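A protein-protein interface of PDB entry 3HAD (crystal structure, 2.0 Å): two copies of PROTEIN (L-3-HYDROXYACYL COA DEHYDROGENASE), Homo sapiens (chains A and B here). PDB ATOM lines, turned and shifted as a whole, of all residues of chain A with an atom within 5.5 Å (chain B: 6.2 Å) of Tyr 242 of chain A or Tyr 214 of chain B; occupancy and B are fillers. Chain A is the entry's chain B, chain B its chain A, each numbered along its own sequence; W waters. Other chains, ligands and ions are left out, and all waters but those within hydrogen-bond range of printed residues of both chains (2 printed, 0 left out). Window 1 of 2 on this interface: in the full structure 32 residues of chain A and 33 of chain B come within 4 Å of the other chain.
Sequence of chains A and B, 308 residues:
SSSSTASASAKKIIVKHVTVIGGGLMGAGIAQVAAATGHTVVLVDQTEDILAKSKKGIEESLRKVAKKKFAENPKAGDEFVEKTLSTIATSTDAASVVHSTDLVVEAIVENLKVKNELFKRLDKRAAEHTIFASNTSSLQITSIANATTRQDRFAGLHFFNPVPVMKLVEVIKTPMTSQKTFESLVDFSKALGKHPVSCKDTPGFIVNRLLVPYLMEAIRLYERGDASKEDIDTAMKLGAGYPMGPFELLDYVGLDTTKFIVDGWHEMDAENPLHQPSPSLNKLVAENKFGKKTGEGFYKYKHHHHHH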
ATOM      1  N   LEU A 210     -20.192 -31.421  13.566  1.00  0.00           N
ATOM      2  CA  LEU A 210     -20.041 -29.968  13.578  1.00  0.00           C
ATOM      3  C   LEU A 210     -20.739 -29.256  12.432  1.00  0.00           C
ATOM      4  O   LEU A 210     -20.982 -28.052  12.511  1.00  0.00           O
ATOM      5  CB  LEU A 210     -18.560 -29.595  13.590  1.00  0.00           C
ATOM      6  CG  LEU A 210     -17.880 -30.152  14.840  1.00  0.00           C
ATOM      7  CD1 LEU A 210     -16.428 -29.759  14.837  1.00  0.00           C
ATOM      8  CD2 LEU A 210     -18.582 -29.609  16.114  1.00  0.00           C
ATOM      9  N   TYR A 214     -25.235 -27.092  12.476  1.00  0.00           N
ATOM     10  CA  TYR A 214     -25.104 -25.719  11.961  1.00  0.00           C
ATOM     11  C   TYR A 214     -26.105 -25.521  10.815  1.00  0.00           C
ATOM     12  O   TYR A 214     -26.769 -24.487  10.727  1.00  0.00           O
ATOM     13  CB  TYR A 214     -23.675 -25.462  11.459  1.00  0.00           C
ATOM     14  CG  TYR A 214     -23.588 -24.570  10.224  1.00  0.00           C
ATOM     15  CD1 TYR A 214     -23.954 -23.228  10.270  1.00  0.00           C
ATOM     16  CD2 TYR A 214     -23.149 -25.090   8.996  1.00  0.00           C
ATOM     17  CE1 TYR A 214     -23.884 -22.419   9.130  1.00  0.00           C
ATOM     18  CE2 TYR A 214     -23.075 -24.291   7.848  1.00  0.00           C
ATOM     19  CZ  TYR A 214     -23.445 -22.963   7.921  1.00  0.00           C
ATOM     20  OH  TYR A 214     -23.396 -22.181   6.792  1.00  0.00           O
ATOM     21  N   MET A 236     -22.905 -16.423   4.863  1.00  0.00           N
ATOM     22  CA  MET A 236     -21.892 -17.405   5.204  1.00  0.00           C
ATOM     23  C   MET A 236     -20.774 -17.490   4.168  1.00  0.00           C
ATOM     24  O   MET A 236     -19.623 -17.749   4.519  1.00  0.00           O
ATOM     25  CB  MET A 236     -22.545 -18.776   5.424  1.00  0.00           C
ATOM     26  CG  MET A 236     -23.691 -18.714   6.436  1.00  0.00           C
ATOM     27  SD  MET A 236     -23.128 -17.892   7.988  1.00  0.00           S
ATOM     28  CE  MET A 236     -21.841 -19.060   8.581  1.00  0.00           C
ATOM     29  N   LYS A 237     -21.088 -17.261   2.894  1.00  0.00           N
ATOM     30  CA  LYS A 237     -20.038 -17.327   1.875  1.00  0.00           C
ATOM     31  C   LYS A 237     -19.042 -16.181   2.006  1.00  0.00           C
ATOM     32  O   LYS A 237     -17.836 -16.400   2.126  1.00  0.00           O
ATOM     33  CB  LYS A 237     -20.643 -17.343   0.467  1.00  0.00           C
ATOM     34  CG  LYS A 237     -21.301 -18.684   0.109  1.00  0.00           C
ATOM     35  CD  LYS A 237     -21.758 -18.756  -1.367  1.00  0.00           C
ATOM     36  CE  LYS A 237     -22.895 -17.782  -1.637  1.00  0.00           C
ATOM     37  NZ  LYS A 237     -23.461 -17.906  -3.023  1.00  0.00           N
ATOM     38  N   LEU A 238     -19.557 -14.957   2.011  1.00  0.00           N
ATOM     39  CA  LEU A 238     -18.720 -13.776   2.099  1.00  0.00           C
ATOM     40  C   LEU A 238     -18.257 -13.451   3.520  1.00  0.00           C
ATOM     41  O   LEU A 238     -17.154 -12.942   3.719  1.00  0.00           O
ATOM     42  CB  LEU A 238     -19.480 -12.579   1.510  1.00  0.00           C
ATOM     43  CG  LEU A 238     -20.001 -12.766   0.076  1.00  0.00           C
ATOM     44  CD1 LEU A 238     -20.579 -11.450  -0.440  1.00  0.00           C
ATOM     45  CD2 LEU A 238     -18.871 -13.231  -0.847  1.00  0.00           C
ATOM     46  N   ALA A 240     -18.113 -15.786   6.174  1.00  0.00           N
ATOM     47  CA  ALA A 240     -17.387 -16.902   6.766  1.00  0.00           C
ATOM     48  C   ALA A 240     -16.461 -17.608   5.761  1.00  0.00           C
ATOM     49  O   ALA A 240     -15.721 -18.524   6.120  1.00  0.00           O
ATOM     50  CB  ALA A 240     -18.374 -17.897   7.353  1.00  0.00           C
ATOM     51  N   GLY A 241     -16.502 -17.177   4.508  1.00  0.00           N
ATOM     52  CA  GLY A 241     -15.638 -17.785   3.510  1.00  0.00           C
ATOM     53  C   GLY A 241     -15.965 -19.235   3.186  1.00  0.00           C
ATOM     54  O   GLY A 241     -15.078 -19.983   2.797  1.00  0.00           O
ATOM     55  N   TYR A 242     -17.219 -19.644   3.356  1.00  0.00           N
ATOM     56  CA  TYR A 242     -17.607 -21.023   3.045  1.00  0.00           C
ATOM     57  C   TYR A 242     -17.829 -21.161   1.521  1.00  0.00           C
ATOM     58  O   TYR A 242     -18.290 -20.234   0.869  1.00  0.00           O
ATOM     59  CB  TYR A 242     -18.895 -21.415   3.800  1.00  0.00           C
ATOM     60  CG  TYR A 242     -18.750 -21.529   5.315  1.00  0.00           C
ATOM     61  CD1 TYR A 242     -17.510 -21.379   5.941  1.00  0.00           C
ATOM     62  CD2 TYR A 242     -19.860 -21.809   6.120  1.00  0.00           C
ATOM     63  CE1 TYR A 242     -17.381 -21.509   7.351  1.00  0.00           C
ATOM     64  CE2 TYR A 242     -19.738 -21.938   7.520  1.00  0.00           C
ATOM     65  CZ  TYR A 242     -18.502 -21.784   8.120  1.00  0.00           C
ATOM     66  OH  TYR A 242     -18.397 -21.900   9.506  1.00  0.00           O
ATOM     67  N   PRO A 243     -17.508 -22.331   0.950  1.00  0.00           N
ATOM     68  CA  PRO A 243     -17.672 -22.558  -0.490  1.00  0.00           C
ATOM     69  C   PRO A 243     -19.121 -22.436  -0.879  1.00  0.00           C
ATOM     70  O   PRO A 243     -19.444 -21.832  -1.894  1.00  0.00           O
ATOM     71  CB  PRO A 243     -17.143 -23.985  -0.675  1.00  0.00           C
ATOM     72  CG  PRO A 243     -16.126 -24.102   0.464  1.00  0.00           C
ATOM     73  CD  PRO A 243     -16.975 -23.542   1.588  1.00  0.00           C
ATOM     74  N   MET A 244     -19.992 -23.016  -0.057  1.00  0.00           N
ATOM     75  CA  MET A 244     -21.420 -22.958  -0.309  1.00  0.00           C
ATOM     76  C   MET A 244     -22.192 -22.434   0.898  1.00  0.00           C
ATOM     77  O   MET A 244     -21.788 -22.648   2.034  1.00  0.00           O
ATOM     78  CB  MET A 244     -21.953 -24.346  -0.649  1.00  0.00           C
ATOM     79  CG  MET A 244     -21.368 -24.981  -1.904  1.00  0.00           C
ATOM     80  SD  MET A 244     -22.082 -26.626  -2.094  1.00  0.00           S
ATOM     81  CE  MET A 244     -23.722 -26.254  -2.300  1.00  0.00           C
ATOM     82  N   GLY A 245     -23.301 -21.752   0.634  1.00  0.00           N
ATOM     83  CA  GLY A 245     -24.144 -21.253   1.701  1.00  0.00           C
ATOM     84  C   GLY A 245     -24.841 -22.468   2.275  1.00  0.00           C
ATOM     85  O   GLY A 245     -24.916 -23.498   1.592  1.00  0.00           O
ATOM     86  N   ARG B 209     -24.447 -15.584  14.571  1.00  0.00           N
ATOM     87  CA  ARG B 209     -25.467 -16.496  15.090  1.00  0.00           C
ATOM     88  C   ARG B 209     -25.298 -17.922  14.570  1.00  0.00           C
ATOM     89  O   ARG B 209     -25.705 -18.876  15.235  1.00  0.00           O
ATOM     90  CB  ARG B 209     -26.866 -15.993  14.740  1.00  0.00           C
ATOM     91  CG  ARG B 209     -28.006 -16.925  15.172  1.00  0.00           C
ATOM     92  CD  ARG B 209     -28.132 -17.056  16.713  1.00  0.00           C
ATOM     93  NE  ARG B 209     -29.273 -17.899  17.104  1.00  0.00           N
ATOM     94  CZ  ARG B 209     -29.294 -19.230  17.021  1.00  0.00           C
ATOM     95  NH1 ARG B 209     -28.225 -19.895  16.586  1.00  0.00           N
ATOM     96  NH2 ARG B 209     -30.378 -19.903  17.395  1.00  0.00           N
ATOM     97  N   LEU B 210     -24.715 -18.073  13.377  1.00  0.00           N
ATOM     98  CA  LEU B 210     -24.510 -19.394  12.793  1.00  0.00           C
ATOM     99  C   LEU B 210     -23.068 -19.833  12.977  1.00  0.00           C
ATOM    100  O   LEU B 210     -22.777 -21.026  13.043  1.00  0.00           O
ATOM    101  CB  LEU B 210     -24.880 -19.376  11.297  1.00  0.00           C
ATOM    102  CG  LEU B 210     -26.370 -19.092  11.077  1.00  0.00           C
ATOM    103  CD1 LEU B 210     -26.717 -19.058   9.581  1.00  0.00           C
ATOM    104  CD2 LEU B 210     -27.179 -20.183  11.783  1.00  0.00           C
ATOM    105  N   LEU B 211     -22.165 -18.867  13.087  1.00  0.00           N
ATOM    106  CA  LEU B 211     -20.761 -19.183  13.268  1.00  0.00           C
ATOM    107  C   LEU B 211     -20.329 -19.502  14.707  1.00  0.00           C
ATOM    108  O   LEU B 211     -19.749 -20.555  14.963  1.00  0.00           O
ATOM    109  CB  LEU B 211     -19.897 -18.035  12.748  1.00  0.00           C
ATOM    110  CG  LEU B 211     -18.381 -18.222  12.865  1.00  0.00           C
ATOM    111  CD1 LEU B 211     -17.913 -19.435  12.026  1.00  0.00           C
ATOM    112  CD2 LEU B 211     -17.689 -16.947  12.399  1.00  0.00           C
ATOM    113  N   VAL B 212     -20.611 -18.597  15.644  1.00  0.00           N
ATOM    114  CA  VAL B 212     -20.172 -18.798  17.029  1.00  0.00           C
ATOM    115  C   VAL B 212     -20.630 -20.081  17.728  1.00  0.00           C
ATOM    116  O   VAL B 212     -19.819 -20.747  18.365  1.00  0.00           O
ATOM    117  CB  VAL B 212     -20.512 -17.562  17.912  1.00  0.00           C
ATOM    118  CG1 VAL B 212     -20.134 -17.845  19.385  1.00  0.00           C
ATOM    119  CG2 VAL B 212     -19.723 -16.327  17.398  1.00  0.00           C
ATOM    120  N   PRO B 213     -21.923 -20.431  17.646  1.00  0.00           N
ATOM    121  CA  PRO B 213     -22.383 -21.659  18.294  1.00  0.00           C
ATOM    122  C   PRO B 213     -21.646 -22.867  17.715  1.00  0.00           C
ATOM    123  O   PRO B 213     -21.412 -23.853  18.418  1.00  0.00           O
ATOM    124  CB  PRO B 213     -23.883 -21.672  17.970  1.00  0.00           C
ATOM    125  CG  PRO B 213     -24.196 -20.201  17.868  1.00  0.00           C
ATOM    126  CD  PRO B 213     -23.056 -19.760  16.994  1.00  0.00           C
ATOM    127  N   TYR B 214     -21.266 -22.787  16.431  1.00  0.00           N
ATOM    128  CA  TYR B 214     -20.534 -23.895  15.817  1.00  0.00           C
ATOM    129  C   TYR B 214     -19.136 -23.982  16.442  1.00  0.00           C
ATOM    130  O   TYR B 214     -18.691 -25.067  16.831  1.00  0.00           O
ATOM    131  CB  TYR B 214     -20.464 -23.716  14.285  1.00  0.00           C
ATOM    132  CG  TYR B 214     -19.166 -24.164  13.647  1.00  0.00           C
ATOM    133  CD1 TYR B 214     -18.736 -25.482  13.732  1.00  0.00           C
ATOM    134  CD2 TYR B 214     -18.356 -23.251  12.970  1.00  0.00           C
ATOM    135  CE1 TYR B 214     -17.522 -25.890  13.165  1.00  0.00           C
ATOM    136  CE2 TYR B 214     -17.145 -23.643  12.398  1.00  0.00           C
ATOM    137  CZ  TYR B 214     -16.733 -24.969  12.506  1.00  0.00           C
ATOM    138  OH  TYR B 214     -15.512 -25.351  11.983  1.00  0.00           O
ATOM    139  N   LEU B 215     -18.455 -22.845  16.568  1.00  0.00           N
ATOM    140  CA  LEU B 215     -17.124 -22.831  17.166  1.00  0.00           C
ATOM    141  C   LEU B 215     -17.180 -23.386  18.602  1.00  0.00           C
ATOM    142  O   LEU B 215     -16.272 -24.101  19.039  1.00  0.00           O
ATOM    143  CB  LEU B 215     -16.557 -21.409  17.166  1.00  0.00           C
ATOM    144  CG  LEU B 215     -16.313 -20.740  15.804  1.00  0.00           C
ATOM    145  CD1 LEU B 215     -15.892 -19.323  16.028  1.00  0.00           C
ATOM    146  CD2 LEU B 215     -15.228 -21.494  15.014  1.00  0.00           C
ATOM    147  N   MET B 216     -18.251 -23.081  19.333  1.00  0.00           N
ATOM    148  CA  MET B 216     -18.381 -23.600  20.696  1.00  0.00           C
ATOM    149  C   MET B 216     -18.501 -25.130  20.661  1.00  0.00           C
ATOM    150  O   MET B 216     -17.881 -25.822  21.471  1.00  0.00           O
ATOM    151  CB  MET B 216     -19.603 -22.985  21.400  1.00  0.00           C
ATOM    152  CG  MET B 216     -19.477 -21.482  21.653  1.00  0.00           C
ATOM    153  SD  MET B 216     -18.074 -21.080  22.717  1.00  0.00           S
ATOM    154  CE  MET B 216     -18.465 -22.159  24.113  1.00  0.00           C
ATOM    155  N   GLU B 217     -19.303 -25.655  19.728  1.00  0.00           N
ATOM    156  CA  GLU B 217     -19.485 -27.104  19.590  1.00  0.00           C
ATOM    157  C   GLU B 217     -18.152 -27.774  19.318  1.00  0.00           C
ATOM    158  O   GLU B 217     -17.891 -28.890  19.779  1.00  0.00           O
ATOM    159  CB  GLU B 217     -20.449 -27.439  18.449  1.00  0.00           C
ATOM    160  CG  GLU B 217     -21.912 -27.275  18.776  1.00  0.00           C
ATOM    161  CD  GLU B 217     -22.333 -28.173  19.929  1.00  0.00           C
ATOM    162  OE1 GLU B 217     -21.944 -27.890  21.078  1.00  0.00           O
ATOM    163  OE2 GLU B 217     -23.031 -29.176  19.686  1.00  0.00           O
ATOM    164  N   ALA B 218     -17.299 -27.084  18.580  1.00  0.00           N
ATOM    165  CA  ALA B 218     -15.988 -27.625  18.256  1.00  0.00           C
ATOM    166  C   ALA B 218     -15.189 -27.729  19.546  1.00  0.00           C
ATOM    167  O   ALA B 218     -14.541 -28.748  19.805  1.00  0.00           O
ATOM    168  CB  ALA B 218     -15.263 -26.712  17.247  1.00  0.00           C
ATOM    169  N   ILE B 219     -15.227 -26.669  20.347  1.00  0.00           N
ATOM    170  CA  ILE B 219     -14.513 -26.662  21.624  1.00  0.00           C
ATOM    171  C   ILE B 219     -15.024 -27.787  22.516  1.00  0.00           C
ATOM    172  O   ILE B 219     -14.244 -28.483  23.153  1.00  0.00           O
ATOM    173  CB  ILE B 219     -14.700 -25.325  22.404  1.00  0.00           C
ATOM    174  CG1 ILE B 219     -14.193 -24.145  21.578  1.00  0.00           C
ATOM    175  CG2 ILE B 219     -13.930 -25.393  23.720  1.00  0.00           C
ATOM    176  CD1 ILE B 219     -14.406 -22.798  22.254  1.00  0.00           C
ATOM    177  N   ILE B 232      -9.589 -31.846  14.343  1.00  0.00           N
ATOM    178  CA  ILE B 232     -10.857 -31.184  14.083  1.00  0.00           C
ATOM    179  C   ILE B 232     -10.656 -30.098  13.022  1.00  0.00           C
ATOM    180  O   ILE B 232     -11.467 -29.960  12.109  1.00  0.00           O
ATOM    181  CB  ILE B 232     -11.440 -30.562  15.374  1.00  0.00           C
ATOM    182  CG1 ILE B 232     -11.733 -31.678  16.384  1.00  0.00           C
ATOM    183  CG2 ILE B 232     -12.719 -29.776  15.067  1.00  0.00           C
ATOM    184  CD1 ILE B 232     -12.336 -31.197  17.688  1.00  0.00           C
ATOM    185  N   MET B 236     -12.466 -30.075   9.325  1.00  0.00           N
ATOM    186  CA  MET B 236     -13.362 -29.053   8.783  1.00  0.00           C
ATOM    187  C   MET B 236     -12.806 -28.369   7.533  1.00  0.00           C
ATOM    188  O   MET B 236     -13.561 -27.950   6.663  1.00  0.00           O
ATOM    189  CB  MET B 236     -13.686 -27.995   9.847  1.00  0.00           C
ATOM    190  CG  MET B 236     -14.310 -28.581  11.092  1.00  0.00           C
ATOM    191  SD  MET B 236     -15.703 -29.671  10.775  1.00  0.00           S
ATOM    192  CE  MET B 236     -16.929 -28.570  10.020  1.00  0.00           C
ATOM    193  N   ALA B 240     -15.178 -29.916   5.108  1.00  0.00           N
ATOM    194  CA  ALA B 240     -16.221 -28.915   4.926  1.00  0.00           C
ATOM    195  C   ALA B 240     -15.776 -27.810   3.982  1.00  0.00           C
ATOM    196  O   ALA B 240     -16.592 -26.987   3.565  1.00  0.00           O
ATOM    197  CB  ALA B 240     -16.618 -28.320   6.278  1.00  0.00           C
ATOM    198  N   GLY B 241     -14.483 -27.786   3.664  1.00  0.00           N
ATOM    199  CA  GLY B 241     -13.958 -26.773   2.760  1.00  0.00           C
ATOM    200  C   GLY B 241     -13.703 -25.408   3.390  1.00  0.00           C
ATOM    201  O   GLY B 241     -13.491 -24.415   2.683  1.00  0.00           O
ATOM    202  N   TYR B 242     -13.705 -25.350   4.720  1.00  0.00           N
ATOM    203  CA  TYR B 242     -13.483 -24.086   5.409  1.00  0.00           C
ATOM    204  C   TYR B 242     -12.039 -23.598   5.299  1.00  0.00           C
ATOM    205  O   TYR B 242     -11.100 -24.398   5.308  1.00  0.00           O
ATOM    206  CB  TYR B 242     -13.849 -24.230   6.889  1.00  0.00           C
ATOM    207  CG  TYR B 242     -15.311 -24.537   7.154  1.00  0.00           C
ATOM    208  CD1 TYR B 242     -16.265 -24.502   6.125  1.00  0.00           C
ATOM    209  CD2 TYR B 242     -15.744 -24.841   8.439  1.00  0.00           C
ATOM    210  CE1 TYR B 242     -17.612 -24.766   6.386  1.00  0.00           C
ATOM    211  CE2 TYR B 242     -17.082 -25.107   8.710  1.00  0.00           C
ATOM    212  CZ  TYR B 242     -18.007 -25.072   7.697  1.00  0.00           C
ATOM    213  OH  TYR B 242     -19.320 -25.364   8.000  1.00  0.00           O
ATOM    214  N   PRO B 243     -11.842 -22.274   5.191  1.00  0.00           N
ATOM    215  CA  PRO B 243     -10.500 -21.687   5.088  1.00  0.00           C
ATOM    216  C   PRO B 243      -9.707 -21.961   6.369  1.00  0.00           C
ATOM    217  O   PRO B 243      -8.496 -22.172   6.357  1.00  0.00           O
ATOM    218  CB  PRO B 243     -10.795 -20.192   4.927  1.00  0.00           C
ATOM    219  CG  PRO B 243     -12.149 -20.195   4.277  1.00  0.00           C
ATOM    220  CD  PRO B 243     -12.855 -21.205   5.133  1.00  0.00           C
ATOM    221  N   MET B 244     -10.407 -21.950   7.484  1.00  0.00           N
ATOM    222  CA  MET B 244      -9.767 -22.193   8.756  1.00  0.00           C
ATOM    223  C   MET B 244     -10.494 -23.212   9.602  1.00  0.00           C
ATOM    224  O   MET B 244     -11.722 -23.246   9.630  1.00  0.00           O
ATOM    225  CB  MET B 244      -9.659 -20.889   9.540  1.00  0.00           C
ATOM    226  CG  MET B 244      -8.539 -19.972   9.081  1.00  0.00           C
ATOM    227  SD  MET B 244      -8.465 -18.468  10.101  1.00  0.00           S
ATOM    228  CE  MET B 244      -9.960 -17.739   9.655  1.00  0.00           C
ATOM    229  N   GLY B 245      -9.723 -24.062  10.271  1.00  0.00           N
ATOM    230  CA  GLY B 245     -10.318 -25.033  11.171  1.00  0.00           C
ATOM    231  C   GLY B 245     -10.903 -24.163  12.286  1.00  0.00           C
ATOM    232  O   GLY B 245     -10.462 -23.031  12.453  1.00  0.00           O
ATOM    233  N   PRO B 246     -11.877 -24.651  13.061  1.00  0.00           N
ATOM    234  CA  PRO B 246     -12.491 -23.867  14.140  1.00  0.00           C
ATOM    235  C   PRO B 246     -11.558 -23.309  15.226  1.00  0.00           C
ATOM    236  O   PRO B 246     -11.769 -22.198  15.712  1.00  0.00           O
ATOM    237  CB  PRO B 246     -13.549 -24.831  14.689  1.00  0.00           C
ATOM    238  CG  PRO B 246     -12.926 -26.185  14.430  1.00  0.00           C
ATOM    239  CD  PRO B 246     -12.501 -25.981  12.989  1.00  0.00           C
ATOM    240  N   LEU B 249      -9.662 -20.448  13.657  1.00  0.00           N
ATOM    241  CA  LEU B 249     -10.534 -19.300  13.495  1.00  0.00           C
ATOM    242  C   LEU B 249     -10.805 -18.638  14.864  1.00  0.00           C
ATOM    243  O   LEU B 249     -10.846 -17.416  14.948  1.00  0.00           O
ATOM    244  CB  LEU B 249     -11.844 -19.707  12.831  1.00  0.00           C
ATOM    245  CG  LEU B 249     -12.822 -18.563  12.544  1.00  0.00           C
ATOM    246  CD1 LEU B 249     -12.157 -17.507  11.687  1.00  0.00           C
ATOM    247  CD2 LEU B 249     -14.059 -19.088  11.838  1.00  0.00           C
HETATM  248  O   HOH W   1     -20.683 -22.684  10.808  1.00  0.00           O
HETATM  249  O   HOH W   2     -20.080 -25.461  10.717  1.00  0.00           O
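The backbone carbonyl oxygen (O) of Met 236 of chain B is in hydrogen-bond range of the backbone NH (N) of Gly 241 of chain B (3.1 Å). The backbone carbonyl oxygen of Met 236 of chain B sits at hydrogen-bond distance from the backbone NH of Tyr 242 of chain B (3.2 Å). The backbone NH of Gly 241 of chain A sits at hydrogen-bond distance from the backbone carbonyl oxygen of Met 236 of chain A (3.2 Å). The backbone carbonyl oxygen (O) of Met 236 of chain A lies within hydrogen-bond range of the backbone NH (N) of Tyr 242 of chain A.
Among the printed residues, merely in contact across the chains: Leu 210 of chain A with Tyr 214 of chain B (3.6 Å), Leu 210 of chain A with Glu 217 of chain B (3.7 Å), Leu 210 of chain A with Ala 218 of chain B (3.8 Å), Leu 210 of chain A with Ile 232 of chain B (3.7 Å), Tyr 214 of chain A with Leu 210 of chain B (3.7 Å), Tyr 214 of chain A with Tyr 242 of chain B (3.9 Å), Gly 241 of chain A with Pro 243 of chain B (3.3 Å), Tyr 242 of chain A with Leu 211 of chain B (3.6 Å), Tyr 242 of chain A with Tyr 214 of chain B (3.6 Å), Tyr 242 of chain A with Tyr 242 of chain B (3.4 Å), Pro 243 of chain A with Ala 240 of chain B (3.99 Å) and Pro 243 of chain A with Gly 241 of chain B (3.5 Å).
Tyr 242 of chain A touches just these residues of chain B: Leu 211 (3.6 Å), Tyr 214 (3.6 Å) and Tyr 242 (3.4 Å). Of the printed residues of chain A, Ala 218 of chain B touches Leu 210 (3.8 Å). Printed residues of chain B within 4 Å of Gly 241 of chain A: Pro 243. Of the printed residues of chain A, Leu 211 of chain B touches Tyr 242 (3.6 Å). Arg 209 of chain B touches none of the printed residues of chain A. The nearest printed residue of chain A that does not touch Ala 218 of chain B is Tyr 242 of chain A (9.6 Å).
Of the 11 printed residues of chain A, 5 touch a printed residue of chain B. Printed residues of chain A that touch a printed residue of chain B: Leu 210, Tyr 214, Gly 241, Tyr 242 and Pro 243. Hydrophobic or aromatic side chains of chain A that line the printed part of chain B: Leu 210, Tyr 214, Tyr 242 and Pro 243. Among the printed residues, no Asp or Glu carboxylate lies within 4 Å of a Lys or Arg side-chain nitrogen of the other chain.
Tyr 214 of chain A touches Tyr 242 of chain B, and with the chains exchanged Tyr 242 of chain A touches Tyr 214 of chain B. Gly 241 of chain A touches Pro 243 of chain B, and with the chains exchanged Pro 243 of chain A touches Gly 241 of chain B. Tyr 242 of chain B touches its own counterpart, Tyr 242 of chain A. Pro 243 of chain A touches Ala 240 of chain B, but with the chains exchanged Ala 240 of chain A does not touch Pro 243 of chain B (4.05 Å). Of the 12 pairs that touch across the chains among the printed residues, 7 have their exchanged pair printed and touching as well.
Water W1 lies within hydrogen-bond range of OH of Tyr 242 of chain A (2.7 Å) and O of Leu 210 of chain B (3.5 Å). Water W2 lies within hydrogen-bond range of the side-chain hydroxyl of Tyr 242 of chain B and the backbone carbonyl oxygen of Leu 210 of chain A.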
